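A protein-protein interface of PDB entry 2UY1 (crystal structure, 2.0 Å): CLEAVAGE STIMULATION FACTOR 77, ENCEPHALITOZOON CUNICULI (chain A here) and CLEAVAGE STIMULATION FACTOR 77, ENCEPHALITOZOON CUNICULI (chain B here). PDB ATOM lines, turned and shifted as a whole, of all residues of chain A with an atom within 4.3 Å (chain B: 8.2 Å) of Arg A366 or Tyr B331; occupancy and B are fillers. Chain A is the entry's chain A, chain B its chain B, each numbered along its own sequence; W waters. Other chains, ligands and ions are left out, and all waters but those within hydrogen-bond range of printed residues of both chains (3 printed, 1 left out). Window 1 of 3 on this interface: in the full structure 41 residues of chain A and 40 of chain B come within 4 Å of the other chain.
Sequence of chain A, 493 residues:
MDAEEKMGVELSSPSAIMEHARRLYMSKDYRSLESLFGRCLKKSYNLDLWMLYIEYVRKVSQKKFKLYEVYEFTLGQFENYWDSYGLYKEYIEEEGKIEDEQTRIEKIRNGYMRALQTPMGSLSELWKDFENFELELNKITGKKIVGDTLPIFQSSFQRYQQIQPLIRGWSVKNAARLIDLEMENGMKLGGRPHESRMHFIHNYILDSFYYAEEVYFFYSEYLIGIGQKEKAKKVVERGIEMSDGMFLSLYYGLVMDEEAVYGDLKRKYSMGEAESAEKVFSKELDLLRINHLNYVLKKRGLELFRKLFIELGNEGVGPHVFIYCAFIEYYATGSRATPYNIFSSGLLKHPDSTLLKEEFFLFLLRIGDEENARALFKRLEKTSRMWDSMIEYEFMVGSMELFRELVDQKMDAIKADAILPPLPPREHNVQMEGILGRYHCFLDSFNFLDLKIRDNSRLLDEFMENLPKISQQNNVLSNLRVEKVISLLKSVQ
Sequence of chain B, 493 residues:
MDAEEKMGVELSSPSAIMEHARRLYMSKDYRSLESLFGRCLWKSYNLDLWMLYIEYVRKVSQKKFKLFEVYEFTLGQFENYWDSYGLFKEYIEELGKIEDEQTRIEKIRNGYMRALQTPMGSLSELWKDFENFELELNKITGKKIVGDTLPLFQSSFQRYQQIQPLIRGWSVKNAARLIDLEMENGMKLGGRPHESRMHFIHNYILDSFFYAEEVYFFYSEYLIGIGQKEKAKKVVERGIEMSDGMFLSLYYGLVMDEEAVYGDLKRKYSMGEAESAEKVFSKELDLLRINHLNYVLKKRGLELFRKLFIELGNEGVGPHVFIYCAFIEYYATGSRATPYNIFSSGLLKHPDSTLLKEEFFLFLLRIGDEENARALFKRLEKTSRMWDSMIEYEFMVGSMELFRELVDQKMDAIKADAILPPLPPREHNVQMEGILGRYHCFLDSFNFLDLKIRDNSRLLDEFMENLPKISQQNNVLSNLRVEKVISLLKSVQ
The side-chain hydroxyl of Tyr A331 lies within hydrogen-bond range of the backbone carbonyl oxygen of Arg B366 (2.6 Å).
The backbone carbonyl oxygen of Arg A366 is in hydrogen-bond range of the side-chain hydroxyl of Tyr B331 (2.9 Å).
The backbone carbonyl oxygen (O) of Ile A367 lies close to the side-chain hydroxyl (OH) of Tyr B330 (2.4 Å).
Among the printed residues, merely in contact across the chains: Tyr A331 with Leu B365, Leu A365 with Tyr B331, Arg A366 with Ile B367, Ile A367 with Arg B366, Tyr A393 with Tyr B331, Met A396 with Ile B328, Met A396 with Tyr B331 and Val A397 with Ile B328.
Printed residues of chain A within 4 Å of Tyr B331: Leu A365, Arg A366, Tyr A393 and Met A396.
Printed residues of chain B within 4 Å of Tyr A331: Leu B365 (3.2 Å) and Arg B366 (2.6 Å).
Printed residues of chain B within 4 Å of Ile A367: Tyr B330 (2.4 Å) and Arg B366 (3.99 Å).
Phe B327 touches none of the printed residues of chain A.
The nearest residue of chain B that does not touch Arg A366 is Arg B366 (4.1 Å).
The nearest printed residue of chain A that does not touch Tyr B331 is Val A397 (4.1 Å).
Hydrophobic or aromatic side chains of chain B within 4 Å of the printed part of chain A: Ile B328, Tyr B330, Tyr B331 and Ile B367.
Hydrophobic or aromatic side chains of chain A that line the printed part of chain B: Tyr A331, Ile A367, Tyr A393, Met A396 and Val A397.
Water W1 bridges O of Met A396 and OH of Tyr B324.
Water W3 bridges OH of Tyr A393 (2.6 Å) and O of Tyr B331 (2.6 Å).
Water W2 bridges the backbone carbonyl oxygen (O) of Tyr B330 (3.0 Å) and the backbone carbonyl oxygen (O) of Gly A368 (3.4 Å).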
ATOM      1  N   TYR A 331     -19.910 -30.691  14.965  1.00  0.00           N
ATOM      2  CA  TYR A 331     -20.764 -31.478  14.058  1.00  0.00           C
ATOM      3  C   TYR A 331     -21.097 -32.835  14.585  1.00  0.00           C
ATOM      4  O   TYR A 331     -22.139 -33.380  14.226  1.00  0.00           O
ATOM      5  CB  TYR A 331     -20.146 -31.518  12.638  1.00  0.00           C
ATOM      6  CG  TYR A 331     -20.303 -30.099  12.029  1.00  0.00           C
ATOM      7  CD1 TYR A 331     -21.560 -29.646  11.607  1.00  0.00           C
ATOM      8  CD2 TYR A 331     -19.235 -29.202  11.988  1.00  0.00           C
ATOM      9  CE1 TYR A 331     -21.762 -28.316  11.089  1.00  0.00           C
ATOM     10  CE2 TYR A 331     -19.410 -27.831  11.437  1.00  0.00           C
ATOM     11  CZ  TYR A 331     -20.703 -27.429  10.997  1.00  0.00           C
ATOM     12  OH  TYR A 331     -20.925 -26.107  10.511  1.00  0.00           O
ATOM     13  N   LEU A 362     -16.211 -16.629  11.609  1.00  0.00           N
ATOM     14  CA  LEU A 362     -17.239 -17.111  10.675  1.00  0.00           C
ATOM     15  C   LEU A 362     -17.979 -18.306  11.218  1.00  0.00           C
ATOM     16  O   LEU A 362     -19.136 -18.449  10.984  1.00  0.00           O
ATOM     17  CB  LEU A 362     -16.695 -17.378   9.282  1.00  0.00           C
ATOM     18  CG  LEU A 362     -16.108 -16.107   8.587  1.00  0.00           C
ATOM     19  CD1 LEU A 362     -15.406 -16.467   7.335  1.00  0.00           C
ATOM     20  CD2 LEU A 362     -17.215 -14.963   8.402  1.00  0.00           C
ATOM     21  N   PHE A 363     -17.292 -19.186  11.909  1.00  0.00           N
ATOM     22  CA  PHE A 363     -17.958 -20.342  12.530  1.00  0.00           C
ATOM     23  C   PHE A 363     -19.070 -19.862  13.470  1.00  0.00           C
ATOM     24  O   PHE A 363     -20.214 -20.314  13.403  1.00  0.00           O
ATOM     25  CB  PHE A 363     -16.891 -21.223  13.272  1.00  0.00           C
ATOM     26  CG  PHE A 363     -17.502 -22.343  14.103  1.00  0.00           C
ATOM     27  CD1 PHE A 363     -18.152 -23.430  13.462  1.00  0.00           C
ATOM     28  CD2 PHE A 363     -17.523 -22.277  15.491  1.00  0.00           C
ATOM     29  CE1 PHE A 363     -18.782 -24.470  14.218  1.00  0.00           C
ATOM     30  CE2 PHE A 363     -18.153 -23.315  16.290  1.00  0.00           C
ATOM     31  CZ  PHE A 363     -18.787 -24.394  15.640  1.00  0.00           C
ATOM     32  N   LEU A 364     -18.742 -18.924  14.364  1.00  0.00           N
ATOM     33  CA  LEU A 364     -19.728 -18.509  15.388  1.00  0.00           C
ATOM     34  C   LEU A 364     -20.961 -17.846  14.753  1.00  0.00           C
ATOM     35  O   LEU A 364     -22.099 -18.147  15.178  1.00  0.00           O
ATOM     36  CB  LEU A 364     -19.118 -17.630  16.476  1.00  0.00           C
ATOM     37  CG  LEU A 364     -18.048 -18.264  17.377  1.00  0.00           C
ATOM     38  CD1 LEU A 364     -17.379 -17.106  18.229  1.00  0.00           C
ATOM     39  CD2 LEU A 364     -18.553 -19.437  18.204  1.00  0.00           C
ATOM     40  N   LEU A 365     -20.742 -17.026  13.696  1.00  0.00           N
ATOM     41  CA  LEU A 365     -21.809 -16.363  12.988  1.00  0.00           C
ATOM     42  C   LEU A 365     -22.719 -17.377  12.244  1.00  0.00           C
ATOM     43  O   LEU A 365     -23.957 -17.241  12.248  1.00  0.00           O
ATOM     44  CB  LEU A 365     -21.264 -15.350  11.957  1.00  0.00           C
ATOM     45  CG  LEU A 365     -21.233 -13.803  11.990  1.00  0.00           C
ATOM     46  CD1 LEU A 365     -21.249 -13.231  10.563  1.00  0.00           C
ATOM     47  CD2 LEU A 365     -22.320 -13.180  12.797  1.00  0.00           C
ATOM     48  N   ARG A 366     -22.102 -18.389  11.631  1.00  0.00           N
ATOM     49  CA  ARG A 366     -22.842 -19.367  10.846  1.00  0.00           C
ATOM     50  C   ARG A 366     -23.745 -20.299  11.645  1.00  0.00           C
ATOM     51  O   ARG A 366     -24.736 -20.733  11.129  1.00  0.00           O
ATOM     52  CB  ARG A 366     -21.938 -20.143   9.870  1.00  0.00           C
ATOM     53  CG  ARG A 366     -21.506 -21.568  10.259  1.00  0.00           C
ATOM     54  CD  ARG A 366     -20.740 -22.314   9.114  1.00  0.00           C
ATOM     55  NE  ARG A 366     -19.843 -21.428   8.369  1.00  0.00           N
ATOM     56  CZ  ARG A 366     -18.508 -21.408   8.493  1.00  0.00           C
ATOM     57  NH1 ARG A 366     -17.850 -22.238   9.349  1.00  0.00           N
ATOM     58  NH2 ARG A 366     -17.808 -20.566   7.729  1.00  0.00           N
ATOM     59  N   ILE A 367     -23.388 -20.632  12.870  1.00  0.00           N
ATOM     60  CA  ILE A 367     -24.171 -21.590  13.647  1.00  0.00           C
ATOM     61  C   ILE A 367     -25.164 -20.873  14.502  1.00  0.00           C
ATOM     62  O   ILE A 367     -26.046 -21.519  15.109  1.00  0.00           O
ATOM     63  CB  ILE A 367     -23.284 -22.535  14.527  1.00  0.00           C
ATOM     64  CG1 ILE A 367     -22.629 -21.741  15.661  1.00  0.00           C
ATOM     65  CG2 ILE A 367     -22.251 -23.305  13.605  1.00  0.00           C
ATOM     66  CD1 ILE A 367     -21.938 -22.600  16.746  1.00  0.00           C
ATOM     67  N   GLY A 368     -25.026 -19.547  14.527  1.00  0.00           N
ATOM     68  CA  GLY A 368     -25.984 -18.645  15.121  1.00  0.00           C
ATOM     69  C   GLY A 368     -25.633 -18.274  16.542  1.00  0.00           C
ATOM     70  O   GLY A 368     -26.528 -17.979  17.328  1.00  0.00           O
ATOM     71  N   GLU A 370     -24.635 -15.702  18.230  1.00  0.00           N
ATOM     72  CA  GLU A 370     -24.514 -14.283  17.951  1.00  0.00           C
ATOM     73  C   GLU A 370     -23.708 -13.463  18.959  1.00  0.00           C
ATOM     74  O   GLU A 370     -22.922 -12.592  18.572  1.00  0.00           O
ATOM     75  CB  GLU A 370     -25.905 -13.663  17.845  1.00  0.00           C
ATOM     76  CG  GLU A 370     -25.884 -12.231  17.344  1.00  0.00           C
ATOM     77  CD  GLU A 370     -27.283 -11.675  17.205  1.00  0.00           C
ATOM     78  OE1 GLU A 370     -27.931 -11.367  18.230  1.00  0.00           O
ATOM     79  OE2 GLU A 370     -27.762 -11.632  16.068  1.00  0.00           O
ATOM     80  N   TYR A 393     -24.422  -9.310   8.211  1.00  0.00           N
ATOM     81  CA  TYR A 393     -25.215  -9.837   9.325  1.00  0.00           C
ATOM     82  C   TYR A 393     -25.987  -8.768  10.044  1.00  0.00           C
ATOM     83  O   TYR A 393     -27.147  -9.009  10.364  1.00  0.00           O
ATOM     84  CB  TYR A 393     -24.349 -10.597  10.328  1.00  0.00           C
ATOM     85  CG  TYR A 393     -25.138 -11.287  11.414  1.00  0.00           C
ATOM     86  CD1 TYR A 393     -25.597 -12.609  11.247  1.00  0.00           C
ATOM     87  CD2 TYR A 393     -25.388 -10.646  12.626  1.00  0.00           C
ATOM     88  CE1 TYR A 393     -26.295 -13.255  12.258  1.00  0.00           C
ATOM     89  CE2 TYR A 393     -26.087 -11.287  13.638  1.00  0.00           C
ATOM     90  CZ  TYR A 393     -26.531 -12.579  13.444  1.00  0.00           C
ATOM     91  OH  TYR A 393     -27.223 -13.208  14.443  1.00  0.00           O
ATOM     92  N   MET A 396     -28.839  -7.537   7.967  1.00  0.00           N
ATOM     93  CA  MET A 396     -29.867  -8.558   7.847  1.00  0.00           C
ATOM     94  C   MET A 396     -30.755  -8.643   9.119  1.00  0.00           C
ATOM     95  O   MET A 396     -31.974  -8.449   9.044  1.00  0.00           O
ATOM     96  CB  MET A 396     -29.215  -9.908   7.519  1.00  0.00           C
ATOM     97  CG  MET A 396     -30.086 -10.825   6.655  1.00  0.00           C
ATOM     98  SD  MET A 396     -29.582 -12.568   6.444  1.00  0.00           S
ATOM     99  CE  MET A 396     -29.308 -13.137   8.162  1.00  0.00           C
ATOM    100  N   VAL A 397     -30.152  -8.915  10.279  1.00  0.00           N
ATOM    101  CA  VAL A 397     -30.908  -9.159  11.496  1.00  0.00           C
ATOM    102  C   VAL A 397     -30.526  -8.260  12.700  1.00  0.00           C
ATOM    103  O   VAL A 397     -30.934  -8.559  13.847  1.00  0.00           O
ATOM    104  CB  VAL A 397     -30.857 -10.677  11.924  1.00  0.00           C
ATOM    105  CG1 VAL A 397     -31.445 -11.567  10.814  1.00  0.00           C
ATOM    106  CG2 VAL A 397     -29.438 -11.110  12.269  1.00  0.00           C
ATOM    107  N   LEU B 302     -40.466  -8.533  14.307  1.00  0.00           N
ATOM    108  CA  LEU B 302     -40.636  -9.815  13.665  1.00  0.00           C
ATOM    109  C   LEU B 302     -42.115 -10.115  13.442  1.00  0.00           C
ATOM    110  O   LEU B 302     -42.510 -10.458  12.320  1.00  0.00           O
ATOM    111  CB  LEU B 302     -39.920 -10.885  14.486  1.00  0.00           C
ATOM    112  CG  LEU B 302     -39.368 -12.211  13.998  1.00  0.00           C
ATOM    113  CD1 LEU B 302     -38.341 -12.122  12.880  1.00  0.00           C
ATOM    114  CD2 LEU B 302     -38.692 -12.699  15.227  1.00  0.00           C
ATOM    115  N   ILE B 323     -35.848 -18.351   0.886  1.00  0.00           N
ATOM    116  CA  ILE B 323     -34.514 -18.561   1.439  1.00  0.00           C
ATOM    117  C   ILE B 323     -34.129 -17.393   2.342  1.00  0.00           C
ATOM    118  O   ILE B 323     -33.583 -17.580   3.424  1.00  0.00           O
ATOM    119  CB  ILE B 323     -33.446 -18.670   0.311  1.00  0.00           C
ATOM    120  CG1 ILE B 323     -33.757 -19.785  -0.704  1.00  0.00           C
ATOM    121  CG2 ILE B 323     -32.010 -18.738   0.874  1.00  0.00           C
ATOM    122  CD1 ILE B 323     -32.755 -19.785  -1.926  1.00  0.00           C
ATOM    123  N   TYR B 324     -34.408 -16.164   1.895  1.00  0.00           N
ATOM    124  CA  TYR B 324     -34.190 -15.016   2.772  1.00  0.00           C
ATOM    125  C   TYR B 324     -34.988 -15.090   4.076  1.00  0.00           C
ATOM    126  O   TYR B 324     -34.447 -14.817   5.152  1.00  0.00           O
ATOM    127  CB  TYR B 324     -34.506 -13.752   2.005  1.00  0.00           C
ATOM    128  CG  TYR B 324     -34.695 -12.573   2.880  1.00  0.00           C
ATOM    129  CD1 TYR B 324     -33.601 -11.816   3.337  1.00  0.00           C
ATOM    130  CD2 TYR B 324     -35.986 -12.211   3.277  1.00  0.00           C
ATOM    131  CE1 TYR B 324     -33.825 -10.752   4.167  1.00  0.00           C
ATOM    132  CE2 TYR B 324     -36.216 -11.159   4.096  1.00  0.00           C
ATOM    133  CZ  TYR B 324     -35.160 -10.422   4.528  1.00  0.00           C
ATOM    134  OH  TYR B 324     -35.445  -9.350   5.345  1.00  0.00           O
ATOM    135  N   CYS B 325     -36.274 -15.442   4.009  1.00  0.00           N
ATOM    136  CA  CYS B 325     -37.116 -15.524   5.247  1.00  0.00           C
ATOM    137  C   CYS B 325     -36.676 -16.617   6.178  1.00  0.00           C
ATOM    138  O   CYS B 325     -36.871 -16.505   7.406  1.00  0.00           O
ATOM    139  CB  CYS B 325     -38.601 -15.775   4.938  1.00  0.00           C
ATOM    140  SG  CYS B 325     -39.402 -14.302   4.232  1.00  0.00           S
ATOM    141  N   ALA B 326     -36.203 -17.727   5.603  1.00  0.00           N
ATOM    142  CA  ALA B 326     -35.723 -18.854   6.436  1.00  0.00           C
ATOM    143  C   ALA B 326     -34.462 -18.441   7.221  1.00  0.00           C
ATOM    144  O   ALA B 326     -34.279 -18.752   8.441  1.00  0.00           O
ATOM    145  CB  ALA B 326     -35.476 -20.078   5.577  1.00  0.00           C
ATOM    146  N   PHE B 327     -33.606 -17.692   6.531  1.00  0.00           N
ATOM    147  CA  PHE B 327     -32.394 -17.182   7.148  1.00  0.00           C
ATOM    148  C   PHE B 327     -32.715 -16.112   8.200  1.00  0.00           C
ATOM    149  O   PHE B 327     -32.082 -16.031   9.190  1.00  0.00           O
ATOM    150  CB  PHE B 327     -31.479 -16.531   6.139  1.00  0.00           C
ATOM    151  CG  PHE B 327     -30.737 -17.469   5.195  1.00  0.00           C
ATOM    152  CD1 PHE B 327     -30.596 -18.839   5.427  1.00  0.00           C
ATOM    153  CD2 PHE B 327     -30.059 -16.897   4.100  1.00  0.00           C
ATOM    154  CE1 PHE B 327     -29.849 -19.641   4.557  1.00  0.00           C
ATOM    155  CE2 PHE B 327     -29.307 -17.709   3.204  1.00  0.00           C
ATOM    156  CZ  PHE B 327     -29.235 -19.081   3.415  1.00  0.00           C
ATOM    157  N   ILE B 328     -33.604 -15.179   7.930  1.00  0.00           N
ATOM    158  CA  ILE B 328     -33.977 -14.284   9.038  1.00  0.00           C
ATOM    159  C   ILE B 328     -34.519 -15.078  10.258  1.00  0.00           C
ATOM    160  O   ILE B 328     -34.270 -14.683  11.375  1.00  0.00           O
ATOM    161  CB  ILE B 328     -35.102 -13.340   8.657  1.00  0.00           C
ATOM    162  CG1 ILE B 328     -34.705 -12.389   7.508  1.00  0.00           C
ATOM    163  CG2 ILE B 328     -35.611 -12.641   9.914  1.00  0.00           C
ATOM    164  CD1 ILE B 328     -33.448 -11.605   7.724  1.00  0.00           C
ATOM    165  N   GLU B 329     -35.282 -16.133  10.022  1.00  0.00           N
ATOM    166  CA  GLU B 329     -35.991 -16.751  11.103  1.00  0.00           C
ATOM    167  C   GLU B 329     -34.959 -17.487  11.881  1.00  0.00           C
ATOM    168  O   GLU B 329     -34.956 -17.416  13.076  1.00  0.00           O
ATOM    169  CB  GLU B 329     -37.122 -17.686  10.664  1.00  0.00           C
ATOM    170  CG  GLU B 329     -38.362 -16.964  10.191  1.00  0.00           C
ATOM    171  CD  GLU B 329     -39.264 -16.409  11.341  1.00  0.00           C
ATOM    172  OE1 GLU B 329     -39.050 -16.668  12.548  1.00  0.00           O
ATOM    173  OE2 GLU B 329     -40.239 -15.712  10.994  1.00  0.00           O
ATOM    174  N   TYR B 330     -34.035 -18.160  11.196  1.00  0.00           N
ATOM    175  CA  TYR B 330     -32.930 -18.831  11.926  1.00  0.00           C
ATOM    176  C   TYR B 330     -32.055 -17.867  12.784  1.00  0.00           C
ATOM    177  O   TYR B 330     -31.922 -18.067  13.975  1.00  0.00           O
ATOM    178  CB  TYR B 330     -32.042 -19.689  11.002  1.00  0.00           C
ATOM    179  CG  TYR B 330     -30.982 -20.383  11.802  1.00  0.00           C
ATOM    180  CD1 TYR B 330     -31.349 -21.329  12.768  1.00  0.00           C
ATOM    181  CD2 TYR B 330     -29.631 -20.035  11.679  1.00  0.00           C
ATOM    182  CE1 TYR B 330     -30.383 -21.968  13.582  1.00  0.00           C
ATOM    183  CE2 TYR B 330     -28.641 -20.684  12.495  1.00  0.00           C
ATOM    184  CZ  TYR B 330     -29.057 -21.627  13.441  1.00  0.00           C
ATOM    185  OH  TYR B 330     -28.137 -22.304  14.234  1.00  0.00           O
ATOM    186  N   TYR B 331     -31.463 -16.840  12.157  1.00  0.00           N
ATOM    187  CA  TYR B 331     -30.524 -15.931  12.859  1.00  0.00           C
ATOM    188  C   TYR B 331     -31.195 -14.991  13.872  1.00  0.00           C
ATOM    189  O   TYR B 331     -30.552 -14.531  14.769  1.00  0.00           O
ATOM    190  CB  TYR B 331     -29.657 -15.166  11.828  1.00  0.00           C
ATOM    191  CG  TYR B 331     -28.782 -16.164  11.148  1.00  0.00           C
ATOM    192  CD1 TYR B 331     -27.691 -16.684  11.806  1.00  0.00           C
ATOM    193  CD2 TYR B 331     -29.108 -16.678   9.893  1.00  0.00           C
ATOM    194  CE1 TYR B 331     -26.927 -17.684  11.233  1.00  0.00           C
ATOM    195  CE2 TYR B 331     -28.344 -17.686   9.304  1.00  0.00           C
ATOM    196  CZ  TYR B 331     -27.245 -18.171   9.986  1.00  0.00           C
ATOM    197  OH  TYR B 331     -26.456 -19.194   9.455  1.00  0.00           O
ATOM    198  N   ALA B 332     -32.495 -14.760  13.729  1.00  0.00           N
ATOM    199  CA  ALA B 332     -33.204 -13.844  14.630  1.00  0.00           C
ATOM    200  C   ALA B 332     -33.702 -14.622  15.861  1.00  0.00           C
ATOM    201  O   ALA B 332     -33.574 -14.168  16.974  1.00  0.00           O
ATOM    202  CB  ALA B 332     -34.360 -13.140  13.903  1.00  0.00           C
ATOM    203  N   THR B 333     -34.181 -15.837  15.641  1.00  0.00           N
ATOM    204  CA  THR B 333     -34.846 -16.607  16.692  1.00  0.00           C
ATOM    205  C   THR B 333     -34.039 -17.832  17.154  1.00  0.00           C
ATOM    206  O   THR B 333     -34.162 -18.241  18.296  1.00  0.00           O
ATOM    207  CB  THR B 333     -36.244 -17.027  16.229  1.00  0.00           C
ATOM    208  OG1 THR B 333     -36.106 -18.082  15.275  1.00  0.00           O
ATOM    209  CG2 THR B 333     -36.951 -15.851  15.606  1.00  0.00           C
ATOM    210  N   GLY B 334     -33.182 -18.395  16.305  1.00  0.00           N
ATOM    211  CA  GLY B 334     -32.556 -19.703  16.623  1.00  0.00           C
ATOM    212  C   GLY B 334     -33.393 -20.975  16.430  1.00  0.00           C
ATOM    213  O   GLY B 334     -32.912 -22.112  16.672  1.00  0.00           O
ATOM    214  N   SER B 335     -34.621 -20.825  15.990  1.00  0.00           N
ATOM    215  CA  SER B 335     -35.429 -22.001  15.590  1.00  0.00           C
ATOM    216  C   SER B 335     -34.768 -22.737  14.407  1.00  0.00           C
ATOM    217  O   SER B 335     -34.341 -22.092  13.433  1.00  0.00           O
ATOM    218  CB  SER B 335     -36.818 -21.559  15.134  1.00  0.00           C
ATOM    219  OG  SER B 335     -37.757 -22.648  15.093  1.00  0.00           O
ATOM    220  N   PRO B 339     -37.263 -22.313   9.851  1.00  0.00           N
ATOM    221  CA  PRO B 339     -36.582 -22.264   8.518  1.00  0.00           C
ATOM    222  C   PRO B 339     -36.749 -23.534   7.693  1.00  0.00           C
ATOM    223  O   PRO B 339     -36.865 -23.439   6.470  1.00  0.00           O
ATOM    224  CB  PRO B 339     -35.100 -21.966   8.831  1.00  0.00           C
ATOM    225  CG  PRO B 339     -34.921 -22.109  10.300  1.00  0.00           C
ATOM    226  CD  PRO B 339     -36.321 -22.070  10.963  1.00  0.00           C
ATOM    227  N   LEU B 362     -27.462 -27.170   2.228  1.00  0.00           N
ATOM    228  CA  LEU B 362     -26.172 -26.715   2.795  1.00  0.00           C
ATOM    229  C   LEU B 362     -26.397 -25.925   4.068  1.00  0.00           C
ATOM    230  O   LEU B 362     -25.564 -25.897   4.980  1.00  0.00           O
ATOM    231  CB  LEU B 362     -25.375 -25.870   1.808  1.00  0.00           C
ATOM    232  CG  LEU B 362     -24.817 -26.576   0.552  1.00  0.00           C
ATOM    233  CD1 LEU B 362     -24.206 -25.539  -0.350  1.00  0.00           C
ATOM    234  CD2 LEU B 362     -23.775 -27.735   0.827  1.00  0.00           C
ATOM    235  N   PHE B 363     -27.556 -25.265   4.113  1.00  0.00           N
ATOM    236  CA  PHE B 363     -28.025 -24.623   5.331  1.00  0.00           C
ATOM    237  C   PHE B 363     -28.241 -25.707   6.383  1.00  0.00           C
ATOM    238  O   PHE B 363     -27.867 -25.563   7.519  1.00  0.00           O
ATOM    239  CB  PHE B 363     -29.379 -23.927   5.103  1.00  0.00           C
ATOM    240  CG  PHE B 363     -30.051 -23.502   6.389  1.00  0.00           C
ATOM    241  CD1 PHE B 363     -29.602 -22.366   7.094  1.00  0.00           C
ATOM    242  CD2 PHE B 363     -31.140 -24.192   6.881  1.00  0.00           C
ATOM    243  CE1 PHE B 363     -30.232 -21.973   8.304  1.00  0.00           C
ATOM    244  CE2 PHE B 363     -31.760 -23.824   8.102  1.00  0.00           C
ATOM    245  CZ  PHE B 363     -31.298 -22.717   8.817  1.00  0.00           C
ATOM    246  N   LEU B 365     -26.912 -28.670   6.722  1.00  0.00           N
ATOM    247  CA  LEU B 365     -25.660 -29.313   7.116  1.00  0.00           C
ATOM    248  C   LEU B 365     -24.793 -28.301   7.928  1.00  0.00           C
ATOM    249  O   LEU B 365     -24.200 -28.659   8.971  1.00  0.00           O
ATOM    250  CB  LEU B 365     -24.956 -29.815   5.846  1.00  0.00           C
ATOM    251  CG  LEU B 365     -23.823 -30.819   5.945  1.00  0.00           C
ATOM    252  CD1 LEU B 365     -24.407 -32.139   6.268  1.00  0.00           C
ATOM    253  CD2 LEU B 365     -23.062 -30.755   4.582  1.00  0.00           C
ATOM    254  N   ARG B 366     -24.798 -27.032   7.526  1.00  0.00           N
ATOM    255  CA  ARG B 366     -23.919 -26.049   8.199  1.00  0.00           C
ATOM    256  C   ARG B 366     -24.304 -25.665   9.605  1.00  0.00           C
ATOM    257  O   ARG B 366     -23.442 -25.420  10.440  1.00  0.00           O
ATOM    258  CB  ARG B 366     -23.683 -24.784   7.398  1.00  0.00           C
ATOM    259  CG  ARG B 366     -24.702 -23.706   7.556  1.00  0.00           C
ATOM    260  CD  ARG B 366     -24.188 -22.348   6.951  1.00  0.00           C
ATOM    261  NE  ARG B 366     -23.865 -22.492   5.516  1.00  0.00           N
ATOM    262  CZ  ARG B 366     -24.706 -22.208   4.511  1.00  0.00           C
ATOM    263  NH1 ARG B 366     -25.937 -21.728   4.793  1.00  0.00           N
ATOM    264  NH2 ARG B 366     -24.303 -22.387   3.222  1.00  0.00           N
ATOM    265  N   ILE B 367     -25.590 -25.591   9.874  1.00  0.00           N
ATOM    266  CA  ILE B 367     -26.046 -25.323  11.259  1.00  0.00           C
ATOM    267  C   ILE B 367     -26.028 -26.553  12.174  1.00  0.00           C
ATOM    268  O   ILE B 367     -26.225 -26.433  13.422  1.00  0.00           O
ATOM    269  CB  ILE B 367     -27.432 -24.744  11.271  1.00  0.00           C
ATOM    270  CG1 ILE B 367     -28.435 -25.775  10.713  1.00  0.00           C
ATOM    271  CG2 ILE B 367     -27.425 -23.387  10.491  1.00  0.00           C
ATOM    272  CD1 ILE B 367     -29.851 -25.695  11.343  1.00  0.00           C
ATOM    273  N   GLY B 368     -25.850 -27.718  11.584  1.00  0.00           N
ATOM    274  CA  GLY B 368     -25.600 -28.903  12.375  1.00  0.00           C
ATOM    275  C   GLY B 368     -26.837 -29.773  12.544  1.00  0.00           C
ATOM    276  O   GLY B 368     -26.870 -30.660  13.401  1.00  0.00           O
HETATM  277  O   HOH W   1     -32.996  -8.257   6.670  1.00  0.00           O
HETATM  278  O   HOH W   2     -29.367 -18.276  15.512  1.00  0.00           O
HETATM  279  O   HOH W   3     -28.163 -15.383  15.501  1.00  0.00           O
